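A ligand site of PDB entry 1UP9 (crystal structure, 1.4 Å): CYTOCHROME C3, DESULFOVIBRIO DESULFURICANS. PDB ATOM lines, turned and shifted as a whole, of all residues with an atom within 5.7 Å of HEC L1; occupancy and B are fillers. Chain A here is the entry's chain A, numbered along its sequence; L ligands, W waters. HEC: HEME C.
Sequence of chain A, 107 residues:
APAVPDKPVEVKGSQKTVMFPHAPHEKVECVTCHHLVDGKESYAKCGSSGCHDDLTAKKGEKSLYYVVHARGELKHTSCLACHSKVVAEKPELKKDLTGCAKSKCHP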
ATOM      1  N   ALA A   1       6.398  -8.369   2.266  1.00  0.00           N
ATOM      2  CA  ALA A   1       5.922  -7.111   1.693  1.00  0.00           C
ATOM      3  C   ALA A   1       6.884  -5.941   1.856  1.00  0.00           C
ATOM      4  O   ALA A   1       7.465  -5.731   2.926  1.00  0.00           O
ATOM      5  CB  ALA A   1       4.606  -6.773   2.394  1.00  0.00           C
ATOM      6  N   PRO A   2       7.061  -5.105   0.841  1.00  0.00           N
ATOM      7  CA  PRO A   2       7.890  -3.894   1.000  1.00  0.00           C
ATOM      8  C   PRO A   2       7.357  -3.005   2.121  1.00  0.00           C
ATOM      9  O   PRO A   2       6.182  -3.107   2.562  1.00  0.00           O
ATOM     10  CB  PRO A   2       7.725  -3.161  -0.324  1.00  0.00           C
ATOM     11  CG  PRO A   2       6.422  -3.718  -0.859  1.00  0.00           C
ATOM     12  CD  PRO A   2       6.504  -5.191  -0.499  1.00  0.00           C
ATOM     13  N   ALA A   3       8.220  -2.103   2.562  1.00  0.00           N
ATOM     14  CA  ALA A   3       7.846  -1.149   3.606  1.00  0.00           C
ATOM     15  C   ALA A   3       6.669  -0.275   3.170  1.00  0.00           C
ATOM     16  O   ALA A   3       6.727   0.241   2.044  1.00  0.00           O
ATOM     17  CB  ALA A   3       8.980  -0.178   3.921  1.00  0.00           C
ATOM     18  N   VAL A   4       5.685  -0.101   4.044  1.00  0.00           N
ATOM     19  CA  VAL A   4       4.633   0.873   3.647  1.00  0.00           C
ATOM     20  C   VAL A   4       5.236   2.265   3.600  1.00  0.00           C
ATOM     21  O   VAL A   4       6.013   2.661   4.462  1.00  0.00           O
ATOM     22  CB  VAL A   4       3.431   0.800   4.595  1.00  0.00           C
ATOM     23  CG1 VAL A   4       3.704   1.449   5.955  1.00  0.00           C
ATOM     24  CG2 VAL A   4       2.168   1.431   4.006  1.00  0.00           C
ATOM     25  N   PRO A   5       4.899   3.043   2.592  1.00  0.00           N
ATOM     26  CA  PRO A   5       5.371   4.447   2.597  1.00  0.00           C
ATOM     27  C   PRO A   5       4.907   5.212   3.853  1.00  0.00           C
ATOM     28  O   PRO A   5       3.744   5.159   4.299  1.00  0.00           O
ATOM     29  CB  PRO A   5       4.758   5.013   1.314  1.00  0.00           C
ATOM     30  CG  PRO A   5       4.545   3.817   0.435  1.00  0.00           C
ATOM     31  CD  PRO A   5       4.119   2.702   1.391  1.00  0.00           C
ATOM     32  N   VAL A   9       2.483   9.639  -1.134  1.00  0.00           N
ATOM     33  CA  VAL A   9       3.167   9.283  -2.395  1.00  0.00           C
ATOM     34  C   VAL A   9       2.386   9.749  -3.591  1.00  0.00           C
ATOM     35  O   VAL A   9       1.142   9.853  -3.522  1.00  0.00           O
ATOM     36  CB  VAL A   9       3.406   7.768  -2.506  1.00  0.00           C
ATOM     37  CG1 VAL A   9       4.341   7.340  -1.359  1.00  0.00           C
ATOM     38  CG2 VAL A   9       2.124   6.932  -2.414  1.00  0.00           C
ATOM     39  N   GLU A  10       3.042  10.008  -4.707  1.00  0.00           N
ATOM     40  CA  GLU A  10       2.342  10.435  -5.901  1.00  0.00           C
ATOM     41  C   GLU A  10       1.548   9.322  -6.594  1.00  0.00           C
ATOM     42  O   GLU A  10       2.081   8.215  -6.829  1.00  0.00           O
ATOM     43  CB  GLU A  10       3.353  10.928  -6.984  1.00  0.00           C
ATOM     44  CG  GLU A  10       3.991  12.256  -6.605  1.00  0.00           C
ATOM     45  CD  GLU A  10       4.641  13.026  -7.737  1.00  0.00           C
ATOM     46  OE1 GLU A  10       5.690  12.395  -8.079  1.00  0.00           O
ATOM     47  OE2 GLU A  10       4.316  14.178  -8.216  1.00  0.00           O
ATOM     48  N   VAL A  11       0.360   9.601  -7.027  1.00  0.00           N
ATOM     49  CA  VAL A  11      -0.367   8.744  -7.962  1.00  0.00           C
ATOM     50  C   VAL A  11      -0.525   9.590  -9.227  1.00  0.00           C
ATOM     51  O   VAL A  11      -1.334  10.507  -9.274  1.00  0.00           O
ATOM     52  CB  VAL A  11      -1.737   8.316  -7.420  1.00  0.00           C
ATOM     53  CG1 VAL A  11      -2.341   7.270  -8.373  1.00  0.00           C
ATOM     54  CG2 VAL A  11      -1.676   7.720  -6.033  1.00  0.00           C
ATOM     55  N   LYS A  12       0.326   9.259 -10.213  1.00  0.00           N
ATOM     56  CA  LYS A  12       0.378  10.032 -11.447  1.00  0.00           C
ATOM     57  C   LYS A  12      -0.654   9.599 -12.477  1.00  0.00           C
ATOM     58  O   LYS A  12      -0.576   8.456 -12.942  1.00  0.00           O
ATOM     59  CB  LYS A  12       1.742   9.946 -12.109  1.00  0.00           C
ATOM     60  CG  LYS A  12       2.794  10.622 -11.253  1.00  0.00           C
ATOM     61  CD  LYS A  12       4.137  10.587 -11.974  1.00  0.00           C
ATOM     62  CE  LYS A  12       5.184  11.255 -11.095  1.00  0.00           C
ATOM     63  NZ  LYS A  12       6.462  11.408 -11.855  1.00  0.00           N
ATOM     64  N   PHE A  20      -1.297  10.270  -2.273  1.00  0.00           N
ATOM     65  CA  PHE A  20      -1.997   9.218  -1.535  1.00  0.00           C
ATOM     66  C   PHE A  20      -1.338   9.052  -0.159  1.00  0.00           C
ATOM     67  O   PHE A  20      -0.125   8.692  -0.096  1.00  0.00           O
ATOM     68  CB  PHE A  20      -1.999   7.884  -2.320  1.00  0.00           C
ATOM     69  CG  PHE A  20      -2.575   6.769  -1.438  1.00  0.00           C
ATOM     70  CD1 PHE A  20      -3.932   6.663  -1.203  1.00  0.00           C
ATOM     71  CD2 PHE A  20      -1.683   5.862  -0.851  1.00  0.00           C
ATOM     72  CE1 PHE A  20      -4.417   5.665  -0.390  1.00  0.00           C
ATOM     73  CE2 PHE A  20      -2.169   4.850  -0.038  1.00  0.00           C
ATOM     74  CZ  PHE A  20      -3.525   4.758   0.197  1.00  0.00           C
ATOM     75  N   HIS A  22      -0.815   6.832   3.138  1.00  0.00           N
ATOM     76  CA  HIS A  22      -1.102   5.526   3.703  1.00  0.00           C
ATOM     77  C   HIS A  22      -1.645   5.640   5.121  1.00  0.00           C
ATOM     78  O   HIS A  22      -2.401   4.729   5.548  1.00  0.00           O
ATOM     79  CB  HIS A  22       0.123   4.593   3.727  1.00  0.00           C
ATOM     80  CG  HIS A  22       0.338   3.946   2.394  1.00  0.00           C
ATOM     81  ND1 HIS A  22       0.957   4.574   1.324  1.00  0.00           N
ATOM     82  CD2 HIS A  22       0.021   2.734   1.915  1.00  0.00           C
ATOM     83  CE1 HIS A  22       1.016   3.752   0.275  1.00  0.00           C
ATOM     84  NE2 HIS A  22       0.434   2.602   0.606  1.00  0.00           N
ATOM     85  N   HIS A  25      -5.149   4.919   6.159  1.00  0.00           N
ATOM     86  CA  HIS A  25      -5.571   3.598   5.688  1.00  0.00           C
ATOM     87  C   HIS A  25      -4.884   2.512   6.478  1.00  0.00           C
ATOM     88  O   HIS A  25      -4.874   1.351   6.034  1.00  0.00           O
ATOM     89  CB  HIS A  25      -5.254   3.494   4.176  1.00  0.00           C
ATOM     90  CG  HIS A  25      -5.955   4.552   3.374  1.00  0.00           C
ATOM     91  ND1 HIS A  25      -5.319   5.736   3.010  1.00  0.00           N
ATOM     92  CD2 HIS A  25      -7.207   4.664   2.909  1.00  0.00           C
ATOM     93  CE1 HIS A  25      -6.145   6.500   2.331  1.00  0.00           C
ATOM     94  NE2 HIS A  25      -7.322   5.867   2.266  1.00  0.00           N
ATOM     95  N   VAL A  28      -6.849  -0.673   6.910  1.00  0.00           N
ATOM     96  CA  VAL A  28      -7.241  -1.333   5.664  1.00  0.00           C
ATOM     97  C   VAL A  28      -6.169  -2.360   5.308  1.00  0.00           C
ATOM     98  O   VAL A  28      -4.961  -2.039   5.286  1.00  0.00           O
ATOM     99  CB  VAL A  28      -7.418  -0.340   4.516  1.00  0.00           C
ATOM    100  CG1 VAL A  28      -7.821  -1.056   3.227  1.00  0.00           C
ATOM    101  CG2 VAL A  28      -8.472   0.693   4.904  1.00  0.00           C
ATOM    102  N   GLU A  29      -6.585  -3.600   5.026  1.00  0.00           N
ATOM    103  CA  GLU A  29      -5.597  -4.588   4.610  1.00  0.00           C
ATOM    104  C   GLU A  29      -4.827  -4.154   3.378  1.00  0.00           C
ATOM    105  O   GLU A  29      -5.463  -3.642   2.454  1.00  0.00           O
ATOM    106  CB  GLU A  29      -6.319  -5.914   4.309  1.00  0.00           C
ATOM    107  CG  GLU A  29      -6.853  -6.577   5.576  1.00  0.00           C
ATOM    108  CD  GLU A  29      -7.597  -7.875   5.310  1.00  0.00           C
ATOM    109  OE1 GLU A  29      -7.719  -8.228   4.118  1.00  0.00           O
ATOM    110  OE2 GLU A  29      -8.076  -8.472   6.312  1.00  0.00           O
ATOM    111  N   CYS A  30      -3.510  -4.395   3.296  1.00  0.00           N
ATOM    112  CA  CYS A  30      -2.760  -3.962   2.112  1.00  0.00           C
ATOM    113  C   CYS A  30      -3.391  -4.513   0.835  1.00  0.00           C
ATOM    114  O   CYS A  30      -3.476  -3.858  -0.175  1.00  0.00           O
ATOM    115  CB  CYS A  30      -1.281  -4.416   2.140  1.00  0.00           C
ATOM    116  SG  CYS A  30      -0.380  -4.219   3.666  1.00  0.00           S
ATOM    117  N   THR A  32      -6.344  -5.094   0.046  1.00  0.00           N
ATOM    118  CA  THR A  32      -7.531  -4.452  -0.531  1.00  0.00           C
ATOM    119  C   THR A  32      -7.177  -3.628  -1.754  1.00  0.00           C
ATOM    120  O   THR A  32      -7.899  -3.606  -2.757  1.00  0.00           O
ATOM    121  CB  THR A  32      -8.147  -3.545   0.537  1.00  0.00           C
ATOM    122  OG1 THR A  32      -8.655  -4.453   1.554  1.00  0.00           O
ATOM    123  CG2 THR A  32      -9.270  -2.714  -0.057  1.00  0.00           C
ATOM    124  N   CYS A  33      -6.027  -2.938  -1.638  1.00  0.00           N
ATOM    125  CA  CYS A  33      -5.558  -2.063  -2.726  1.00  0.00           C
ATOM    126  C   CYS A  33      -4.522  -2.784  -3.603  1.00  0.00           C
ATOM    127  O   CYS A  33      -4.687  -2.838  -4.808  1.00  0.00           O
ATOM    128  CB  CYS A  33      -4.965  -0.778  -2.135  1.00  0.00           C
ATOM    129  SG  CYS A  33      -6.258   0.072  -1.188  1.00  0.00           S
ATOM    130  N   HIS A  34      -3.497  -3.252  -2.913  1.00  0.00           N
ATOM    131  CA  HIS A  34      -2.426  -3.999  -3.588  1.00  0.00           C
ATOM    132  C   HIS A  34      -2.900  -5.421  -3.775  1.00  0.00           C
ATOM    133  O   HIS A  34      -2.451  -6.369  -3.101  1.00  0.00           O
ATOM    134  CB  HIS A  34      -1.165  -3.940  -2.751  1.00  0.00           C
ATOM    135  CG  HIS A  34      -0.649  -2.554  -2.553  1.00  0.00           C
ATOM    136  ND1 HIS A  34       0.012  -1.830  -3.544  1.00  0.00           N
ATOM    137  CD2 HIS A  34      -0.680  -1.741  -1.475  1.00  0.00           C
ATOM    138  CE1 HIS A  34       0.351  -0.633  -3.056  1.00  0.00           C
ATOM    139  NE2 HIS A  34      -0.069  -0.549  -1.812  1.00  0.00           N
ATOM    140  N   TYR A  43       3.004  -5.327  -5.173  1.00  0.00           N
ATOM    141  CA  TYR A  43       2.965  -3.989  -4.610  1.00  0.00           C
ATOM    142  C   TYR A  43       3.419  -2.952  -5.611  1.00  0.00           C
ATOM    143  O   TYR A  43       3.737  -1.802  -5.258  1.00  0.00           O
ATOM    144  CB  TYR A  43       3.881  -3.993  -3.390  1.00  0.00           C
ATOM    145  CG  TYR A  43       3.364  -4.719  -2.179  1.00  0.00           C
ATOM    146  CD1 TYR A  43       3.689  -6.030  -1.943  1.00  0.00           C
ATOM    147  CD2 TYR A  43       2.517  -4.083  -1.267  1.00  0.00           C
ATOM    148  CE1 TYR A  43       3.219  -6.700  -0.843  1.00  0.00           C
ATOM    149  CE2 TYR A  43       2.039  -4.760  -0.158  1.00  0.00           C
ATOM    150  CZ  TYR A  43       2.383  -6.065   0.067  1.00  0.00           C
ATOM    151  OH  TYR A  43       1.943  -6.771   1.167  1.00  0.00           O
ATOM    152  N   ALA A  44       3.483  -3.346  -6.883  1.00  0.00           N
ATOM    153  CA  ALA A  44       3.919  -2.400  -7.904  1.00  0.00           C
ATOM    154  C   ALA A  44       2.908  -1.262  -8.059  1.00  0.00           C
ATOM    155  O   ALA A  44       1.752  -1.328  -7.717  1.00  0.00           O
ATOM    156  CB  ALA A  44       4.102  -3.096  -9.238  1.00  0.00           C
ATOM    157  N   LYS A  45       3.398  -0.161  -8.646  1.00  0.00           N
ATOM    158  CA  LYS A  45       2.507   0.974  -8.859  1.00  0.00           C
ATOM    159  C   LYS A  45       1.351   0.557  -9.758  1.00  0.00           C
ATOM    160  O   LYS A  45       1.479  -0.213 -10.690  1.00  0.00           O
ATOM    161  CB  LYS A  45       3.264   2.156  -9.454  1.00  0.00           C
ATOM    162  CG  LYS A  45       4.449   2.607  -8.611  1.00  0.00           C
ATOM    163  CD  LYS A  45       5.220   3.740  -9.276  1.00  0.00           C
ATOM    164  CE  LYS A  45       6.067   4.485  -8.248  1.00  0.00           C
ATOM    165  NZ  LYS A  45       7.338   4.947  -8.869  1.00  0.00           N
ATOM    166  N   CYS A  46       0.180   1.086  -9.398  1.00  0.00           N
ATOM    167  CA  CYS A  46      -1.061   0.684 -10.045  1.00  0.00           C
ATOM    168  C   CYS A  46      -0.998   0.887 -11.549  1.00  0.00           C
ATOM    169  O   CYS A  46      -1.541   0.063 -12.308  1.00  0.00           O
ATOM    170  CB  CYS A  46      -2.269   1.431  -9.476  1.00  0.00           C
ATOM    171  SG  CYS A  46      -2.314   1.633  -7.691  1.00  0.00           S
ATOM    172  N   GLY A  47      -0.343   1.972 -11.993  1.00  0.00           N
ATOM    173  CA  GLY A  47      -0.227   2.313 -13.376  1.00  0.00           C
ATOM    174  C   GLY A  47       1.003   1.744 -14.055  1.00  0.00           C
ATOM    175  O   GLY A  47       1.317   2.187 -15.175  1.00  0.00           O
ATOM    176  N   LEU A  64      -6.417   3.510 -15.306  1.00  0.00           N
ATOM    177  CA  LEU A  64      -6.110   3.980 -13.951  1.00  0.00           C
ATOM    178  C   LEU A  64      -7.274   4.804 -13.426  1.00  0.00           C
ATOM    179  O   LEU A  64      -7.692   4.712 -12.281  1.00  0.00           O
ATOM    180  CB  LEU A  64      -4.756   4.734 -13.938  1.00  0.00           C
ATOM    181  CG  LEU A  64      -4.303   5.149 -12.523  1.00  0.00           C
ATOM    182  CD1 LEU A  64      -4.145   3.906 -11.638  1.00  0.00           C
ATOM    183  CD2 LEU A  64      -3.001   5.942 -12.606  1.00  0.00           C
HETATM  184 FE   HEC L   1       0.215   0.993  -0.593  1.00  0.00          FE
HETATM  185  CHA HEC L   1       2.079   2.807  -2.819  1.00  0.00           C
HETATM  186  CHB HEC L   1       2.936  -0.732   0.305  1.00  0.00           C
HETATM  187  CHC HEC L   1      -1.572  -0.411   1.995  1.00  0.00           C
HETATM  188  CHD HEC L   1      -2.708   2.209  -1.935  1.00  0.00           C
HETATM  189  NA  HEC L   1       2.157   1.080  -1.093  1.00  0.00           N
HETATM  190  C1A HEC L   1       2.751   1.836  -2.111  1.00  0.00           C
HETATM  191  C2A HEC L   1       4.140   1.437  -2.256  1.00  0.00           C
HETATM  192  C3A HEC L   1       4.372   0.474  -1.366  1.00  0.00           C
HETATM  193  C4A HEC L   1       3.129   0.222  -0.660  1.00  0.00           C
HETATM  194  CMA HEC L   1       5.700  -0.254  -1.056  1.00  0.00           C
HETATM  195  CAA HEC L   1       5.106   2.016  -3.283  1.00  0.00           C
HETATM  196  CBA HEC L   1       5.020   1.239  -4.609  1.00  0.00           C
HETATM  197  CGA HEC L   1       3.761   1.575  -5.409  1.00  0.00           C
HETATM  198  O1A HEC L   1       2.869   0.691  -5.487  1.00  0.00           O
HETATM  199  O2A HEC L   1       3.739   2.737  -5.907  1.00  0.00           O
HETATM  200  NB  HEC L   1       0.647  -0.263   0.904  1.00  0.00           N
HETATM  201  C1B HEC L   1       1.824  -0.934   1.084  1.00  0.00           C
HETATM  202  C2B HEC L   1       1.706  -1.865   2.192  1.00  0.00           C
HETATM  203  C3B HEC L   1       0.457  -1.732   2.676  1.00  0.00           C
HETATM  204  C4B HEC L   1      -0.232  -0.766   1.848  1.00  0.00           C
HETATM  205  CMB HEC L   1       2.851  -2.752   2.664  1.00  0.00           C
HETATM  206  CAB HEC L   1      -0.218  -2.409   3.867  1.00  0.00           C
HETATM  207  CBB HEC L   1       0.592  -2.212   5.174  1.00  0.00           C
HETATM  208  NC  HEC L   1      -1.716   0.920  -0.095  1.00  0.00           N
HETATM  209  C1C HEC L   1      -2.270   0.302   1.033  1.00  0.00           C
HETATM  210  C2C HEC L   1      -3.700   0.478   1.037  1.00  0.00           C
HETATM  211  C3C HEC L   1      -3.998   1.157  -0.054  1.00  0.00           C
HETATM  212  C4C HEC L   1      -2.795   1.467  -0.765  1.00  0.00           C
HETATM  213  CMC HEC L   1      -4.580  -0.133   2.131  1.00  0.00           C
HETATM  214  CAC HEC L   1      -5.381   1.551  -0.592  1.00  0.00           C
HETATM  215  CBC HEC L   1      -6.322   2.245   0.430  1.00  0.00           C
HETATM  216  ND  HEC L   1      -0.210   2.227  -2.099  1.00  0.00           N
HETATM  217  C1D HEC L   1      -1.500   2.588  -2.500  1.00  0.00           C
HETATM  218  C2D HEC L   1      -1.387   3.491  -3.622  1.00  0.00           C
HETATM  219  C3D HEC L   1      -0.066   3.670  -3.891  1.00  0.00           C
HETATM  220  C4D HEC L   1       0.681   2.884  -2.926  1.00  0.00           C
HETATM  221  CMD HEC L   1      -2.578   4.093  -4.344  1.00  0.00           C
HETATM  222  CAD HEC L   1       0.550   4.519  -5.006  1.00  0.00           C
HETATM  223  CBD HEC L   1       0.873   3.618  -6.232  1.00  0.00           C
HETATM  224  CGD HEC L   1       1.150   4.362  -7.512  1.00  0.00           C
HETATM  225  O1D HEC L   1       0.604   3.895  -8.522  1.00  0.00           O
HETATM  226  O2D HEC L   1       1.858   5.353  -7.491  1.00  0.00           O
HETATM  227 FE   HEC L   2      -9.010   6.582   1.465  1.00  0.00          FE
HETATM  228  CHA HEC L   2      -9.045   8.861   4.000  1.00  0.00           C
HETATM  229  CHB HEC L   2      -7.273   8.814  -0.527  1.00  0.00           C
HETATM  230  CHC HEC L   2      -8.757   4.236  -1.006  1.00  0.00           C
HETATM  231  CHD HEC L   2     -10.788   4.393   3.409  1.00  0.00           C
HETATM  232  NA  HEC L   2      -8.361   8.436   1.679  1.00  0.00           N
HETATM  233  C1A HEC L   2      -8.454   9.230   2.807  1.00  0.00           C
HETATM  234  C2A HEC L   2      -7.891  10.542   2.549  1.00  0.00           C
HETATM  235  C3A HEC L   2      -7.376  10.533   1.307  1.00  0.00           C
HETATM  236  C4A HEC L   2      -7.643   9.214   0.749  1.00  0.00           C
HETATM  237  CMA HEC L   2      -6.674  11.663   0.563  1.00  0.00           C
HETATM  238  CAA HEC L   2      -8.023  11.722   3.536  1.00  0.00           C
HETATM  239  CBA HEC L   2      -6.751  11.879   4.402  1.00  0.00           C
HETATM  240  CGA HEC L   2      -6.837  13.202   5.164  1.00  0.00           C
HETATM  241  O1A HEC L   2      -7.119  13.104   6.365  1.00  0.00           O
HETATM  242  O2A HEC L   2      -6.640  14.237   4.519  1.00  0.00           O
HETATM  243  NB  HEC L   2      -8.182   6.547  -0.336  1.00  0.00           N
HETATM  244  C1B HEC L   2      -7.553   7.566  -1.065  1.00  0.00           C
HETATM  245  C2B HEC L   2      -7.220   7.127  -2.407  1.00  0.00           C
HETATM  246  C3B HEC L   2      -7.614   5.841  -2.492  1.00  0.00           C
HETATM  247  C4B HEC L   2      -8.218   5.485  -1.223  1.00  0.00           C
HETATM  248  CMB HEC L   2      -6.588   8.044  -3.466  1.00  0.00           C
HETATM  249  CAB HEC L   2      -7.540   4.843  -3.628  1.00  0.00           C
HETATM  250  CBB HEC L   2      -6.072   4.658  -4.135  1.00  0.00           C
HETATM  251  NC  HEC L   2      -9.672   4.728   1.239  1.00  0.00           N
HETATM  252  C1C HEC L   2      -9.480   3.915   0.146  1.00  0.00           C
HETATM  253  C2C HEC L   2     -10.137   2.629   0.346  1.00  0.00           C
HETATM  254  C3C HEC L   2     -10.738   2.670   1.565  1.00  0.00           C
HETATM  255  C4C HEC L   2     -10.418   3.980   2.132  1.00  0.00           C
HETATM  256  CMC HEC L   2     -10.126   1.533  -0.734  1.00  0.00           C
HETATM  257  CAC HEC L   2     -11.613   1.660   2.293  1.00  0.00           C
HETATM  258  CBC HEC L   2     -11.366   0.190   1.992  1.00  0.00           C
HETATM  259  ND  HEC L   2      -9.803   6.636   3.280  1.00  0.00           N
HETATM  260  C1D HEC L   2     -10.453   5.611   3.963  1.00  0.00           C
HETATM  261  C2D HEC L   2     -10.735   5.999   5.313  1.00  0.00           C
HETATM  262  C3D HEC L   2     -10.245   7.230   5.469  1.00  0.00           C
HETATM  263  C4D HEC L   2      -9.649   7.649   4.240  1.00  0.00           C
HETATM  264  CMD HEC L   2     -11.403   5.069   6.351  1.00  0.00           C
HETATM  265  CAD HEC L   2     -10.253   8.011   6.788  1.00  0.00           C
HETATM  266  CBD HEC L   2     -11.650   8.636   6.999  1.00  0.00           C
HETATM  267  CGD HEC L   2     -11.766   9.143   8.430  1.00  0.00           C
HETATM  268  O1D HEC L   2     -10.985  10.057   8.737  1.00  0.00           O
HETATM  269  O2D HEC L   2     -12.612   8.592   9.169  1.00  0.00           O
HETATM  270 FE   HEC L   3      -5.306  -3.704 -10.324  1.00  0.00          FE
HETATM  271  CHA HEC L   3      -8.143  -5.141 -11.457  1.00  0.00           C
HETATM  272  CHB HEC L   3      -7.125  -1.465  -8.535  1.00  0.00           C
HETATM  273  CHC HEC L   3      -2.434  -2.535  -8.863  1.00  0.00           C
HETATM  274  CHD HEC L   3      -3.412  -5.708 -12.407  1.00  0.00           C
HETATM  275  NA  HEC L   3      -7.246  -3.378 -10.018  1.00  0.00           N
HETATM  276  C1A HEC L   3      -8.277  -4.044 -10.603  1.00  0.00           C
HETATM  277  C2A HEC L   3      -9.546  -3.463 -10.183  1.00  0.00           C
HETATM  278  C3A HEC L   3      -9.289  -2.495  -9.305  1.00  0.00           C
HETATM  279  C4A HEC L   3      -7.842  -2.390  -9.234  1.00  0.00           C
HETATM  280  CMA HEC L   3     -10.266  -1.605  -8.510  1.00  0.00           C
HETATM  281  CAA HEC L   3     -10.900  -3.954 -10.727  1.00  0.00           C
HETATM  282  CBA HEC L   3     -11.188  -3.378 -12.120  1.00  0.00           C
HETATM  283  CGA HEC L   3     -12.446  -3.964 -12.725  1.00  0.00           C
HETATM  284  O1A HEC L   3     -13.164  -4.697 -12.026  1.00  0.00           O
HETATM  285  O2A HEC L   3     -12.666  -3.663 -13.908  1.00  0.00           O
HETATM  286  NB  HEC L   3      -4.870  -2.275  -9.004  1.00  0.00           N
HETATM  287  C1B HEC L   3      -5.772  -1.414  -8.372  1.00  0.00           C
HETATM  288  C2B HEC L   3      -5.052  -0.427  -7.577  1.00  0.00           C
HETATM  289  C3B HEC L   3      -3.737  -0.753  -7.704  1.00  0.00           C
HETATM  290  C4B HEC L   3      -3.623  -1.899  -8.548  1.00  0.00           C
HETATM  291  CMB HEC L   3      -5.739   0.707  -6.813  1.00  0.00           C
HETATM  292  CAB HEC L   3      -2.538  -0.045  -7.062  1.00  0.00           C
HETATM  293  CBB HEC L   3      -2.653   0.079  -5.524  1.00  0.00           C
HETATM  294  NC  HEC L   3      -3.355  -4.017 -10.588  1.00  0.00           N
HETATM  295  C1C HEC L   3      -2.311  -3.445  -9.885  1.00  0.00           C
HETATM  296  C2C HEC L   3      -1.059  -3.918 -10.393  1.00  0.00           C
HETATM  297  C3C HEC L   3      -1.328  -4.742 -11.439  1.00  0.00           C
HETATM  298  C4C HEC L   3      -2.748  -4.869 -11.523  1.00  0.00           C
HETATM  299  CMC HEC L   3       0.331  -3.499  -9.859  1.00  0.00           C
HETATM  300  CAC HEC L   3      -0.336  -5.396 -12.428  1.00  0.00           C
HETATM  301  CBC HEC L   3       0.685  -6.337 -11.769  1.00  0.00           C
HETATM  302  ND  HEC L   3      -5.694  -5.128 -11.661  1.00  0.00           N
HETATM  303  C1D HEC L   3      -4.800  -5.874 -12.391  1.00  0.00           C
HETATM  304  C2D HEC L   3      -5.508  -6.897 -13.124  1.00  0.00           C
HETATM  305  C3D HEC L   3      -6.825  -6.751 -12.848  1.00  0.00           C
HETATM  306  C4D HEC L   3      -6.960  -5.619 -11.957  1.00  0.00           C
HETATM  307  CMD HEC L   3      -4.793  -7.946 -14.008  1.00  0.00           C
HETATM  308  CAD HEC L   3      -8.015  -7.567 -13.386  1.00  0.00           C
HETATM  309  CBD HEC L   3      -8.305  -8.862 -12.617  1.00  0.00           C
HETATM  310  CGD HEC L   3      -8.750  -8.710 -11.177  1.00  0.00           C
HETATM  311  O1D HEC L   3      -9.898  -8.279 -10.926  1.00  0.00           O
HETATM  312  O2D HEC L   3      -7.901  -9.074 -10.328  1.00  0.00           O
HETATM  313  O   HOH W   1       0.761   0.239   7.499  1.00  0.00           O
HETATM  314  O   HOH W   2       8.503   1.933  -2.784  1.00  0.00           O
HETATM  315  O   HOH W   3       5.099   5.011  -4.808  1.00  0.00           O
HETATM  316  O   HOH W   4       2.141   6.896  -9.761  1.00  0.00           O
HETATM  317  O   HOH W   5      -2.598  -0.502   5.145  1.00  0.00           O
HETATM  318  O   HOH W   6       0.525   4.191 -11.196  1.00  0.00           O
HETATM  319  O   HOH W   7       4.522   6.962  -6.509  1.00  0.00           O
HETATM  320  O   HOH W   8      -1.633  -1.378   7.341  1.00  0.00           O
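A carbon (CAC) of HEC L1 is covalently linked to the side-chain sulfur of Cys 33. SG of Cys 30 is covalently linked to CAB of HEC L1 (1.8 Å). NE2 of His 34 binds FE of HEC L1 (2.0 Å). NE2 of His 22 binds FE of HEC L1 (2.0 Å). The backbone carbonyl oxygen (O) of Tyr 43 sits close to an oxygen (O1A) of HEC L1 (2.6 Å). O1A of HEC L1 lies within hydrogen-bond range of N of Lys 45, at 3.3 Å. An oxygen (O2D) of HEC L1 lies close to the backbone carbonyl oxygen (O) of Glu 10, 2.9 Å away. The backbone NH (N) of Cys 46 is in hydrogen-bond range of an oxygen (O1D) of HEC L1, 3.0 Å away. A ring nitrogen (NE2) of His 25 binds an iron atom (FE) of HEC L2 (2.0 Å). A carbon (CAB) of HEC L3 is bonded to the side-chain sulfur (SG) of Cys 46 (1.8 Å).
NZ of Lys 12 is in salt-bridge range of OE1 of Glu 10. O of Val 9 lies within hydrogen-bond range of N of Phe 20, at 2.8 Å. The backbone carbonyl oxygen (O) of Glu 29 lies close to the side-chain hydroxyl (OG1) of Thr 32 (3.4 Å).
The backbone carbonyl oxygen (O) of Ala 44 lies close to an oxygen (O1A) of HEC L1, at 3.2 Å. Residues that only touch HEC L1: Phe 20, Ala 3, Pro 2, Pro 5, Val 28, His 25, Glu 29, Val 4 and Val 9. Hydrophobic or aromatic side chains that line HEC L1: Pro 2, Val 4, Pro 5, Val 9, Phe 20, His 22, His 25, Val 28, His 34 and Tyr 43. 18 residues have an atom within 4 Å of HEC L1: Pro 2, Ala 3, Val 4, Pro 5, Val 9, Glu 10, Phe 20, His 22, His 25, Val 28, Glu 29, Cys 30, Cys 33, His 34, Tyr 43, Ala 44, Lys 45 and Cys 46. The nearest printed residue that does not touch HEC L1 is Val 11 (4.03 Å).
Water W6 lies within hydrogen-bond range of the backbone NH (N) of Gly 47 (2.5 Å) and an oxygen (O1D) of HEC L1 (2.7 Å). Water W4 lies within hydrogen-bond range of O2D of HEC L1 (2.8 Å), N of Lys 12 (3.0 Å) and O of Glu 10 (3.2 Å). Water W7 lies within hydrogen-bond range of O of Glu 10 (2.8 Å) and O2D of HEC L1 (3.3 Å).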
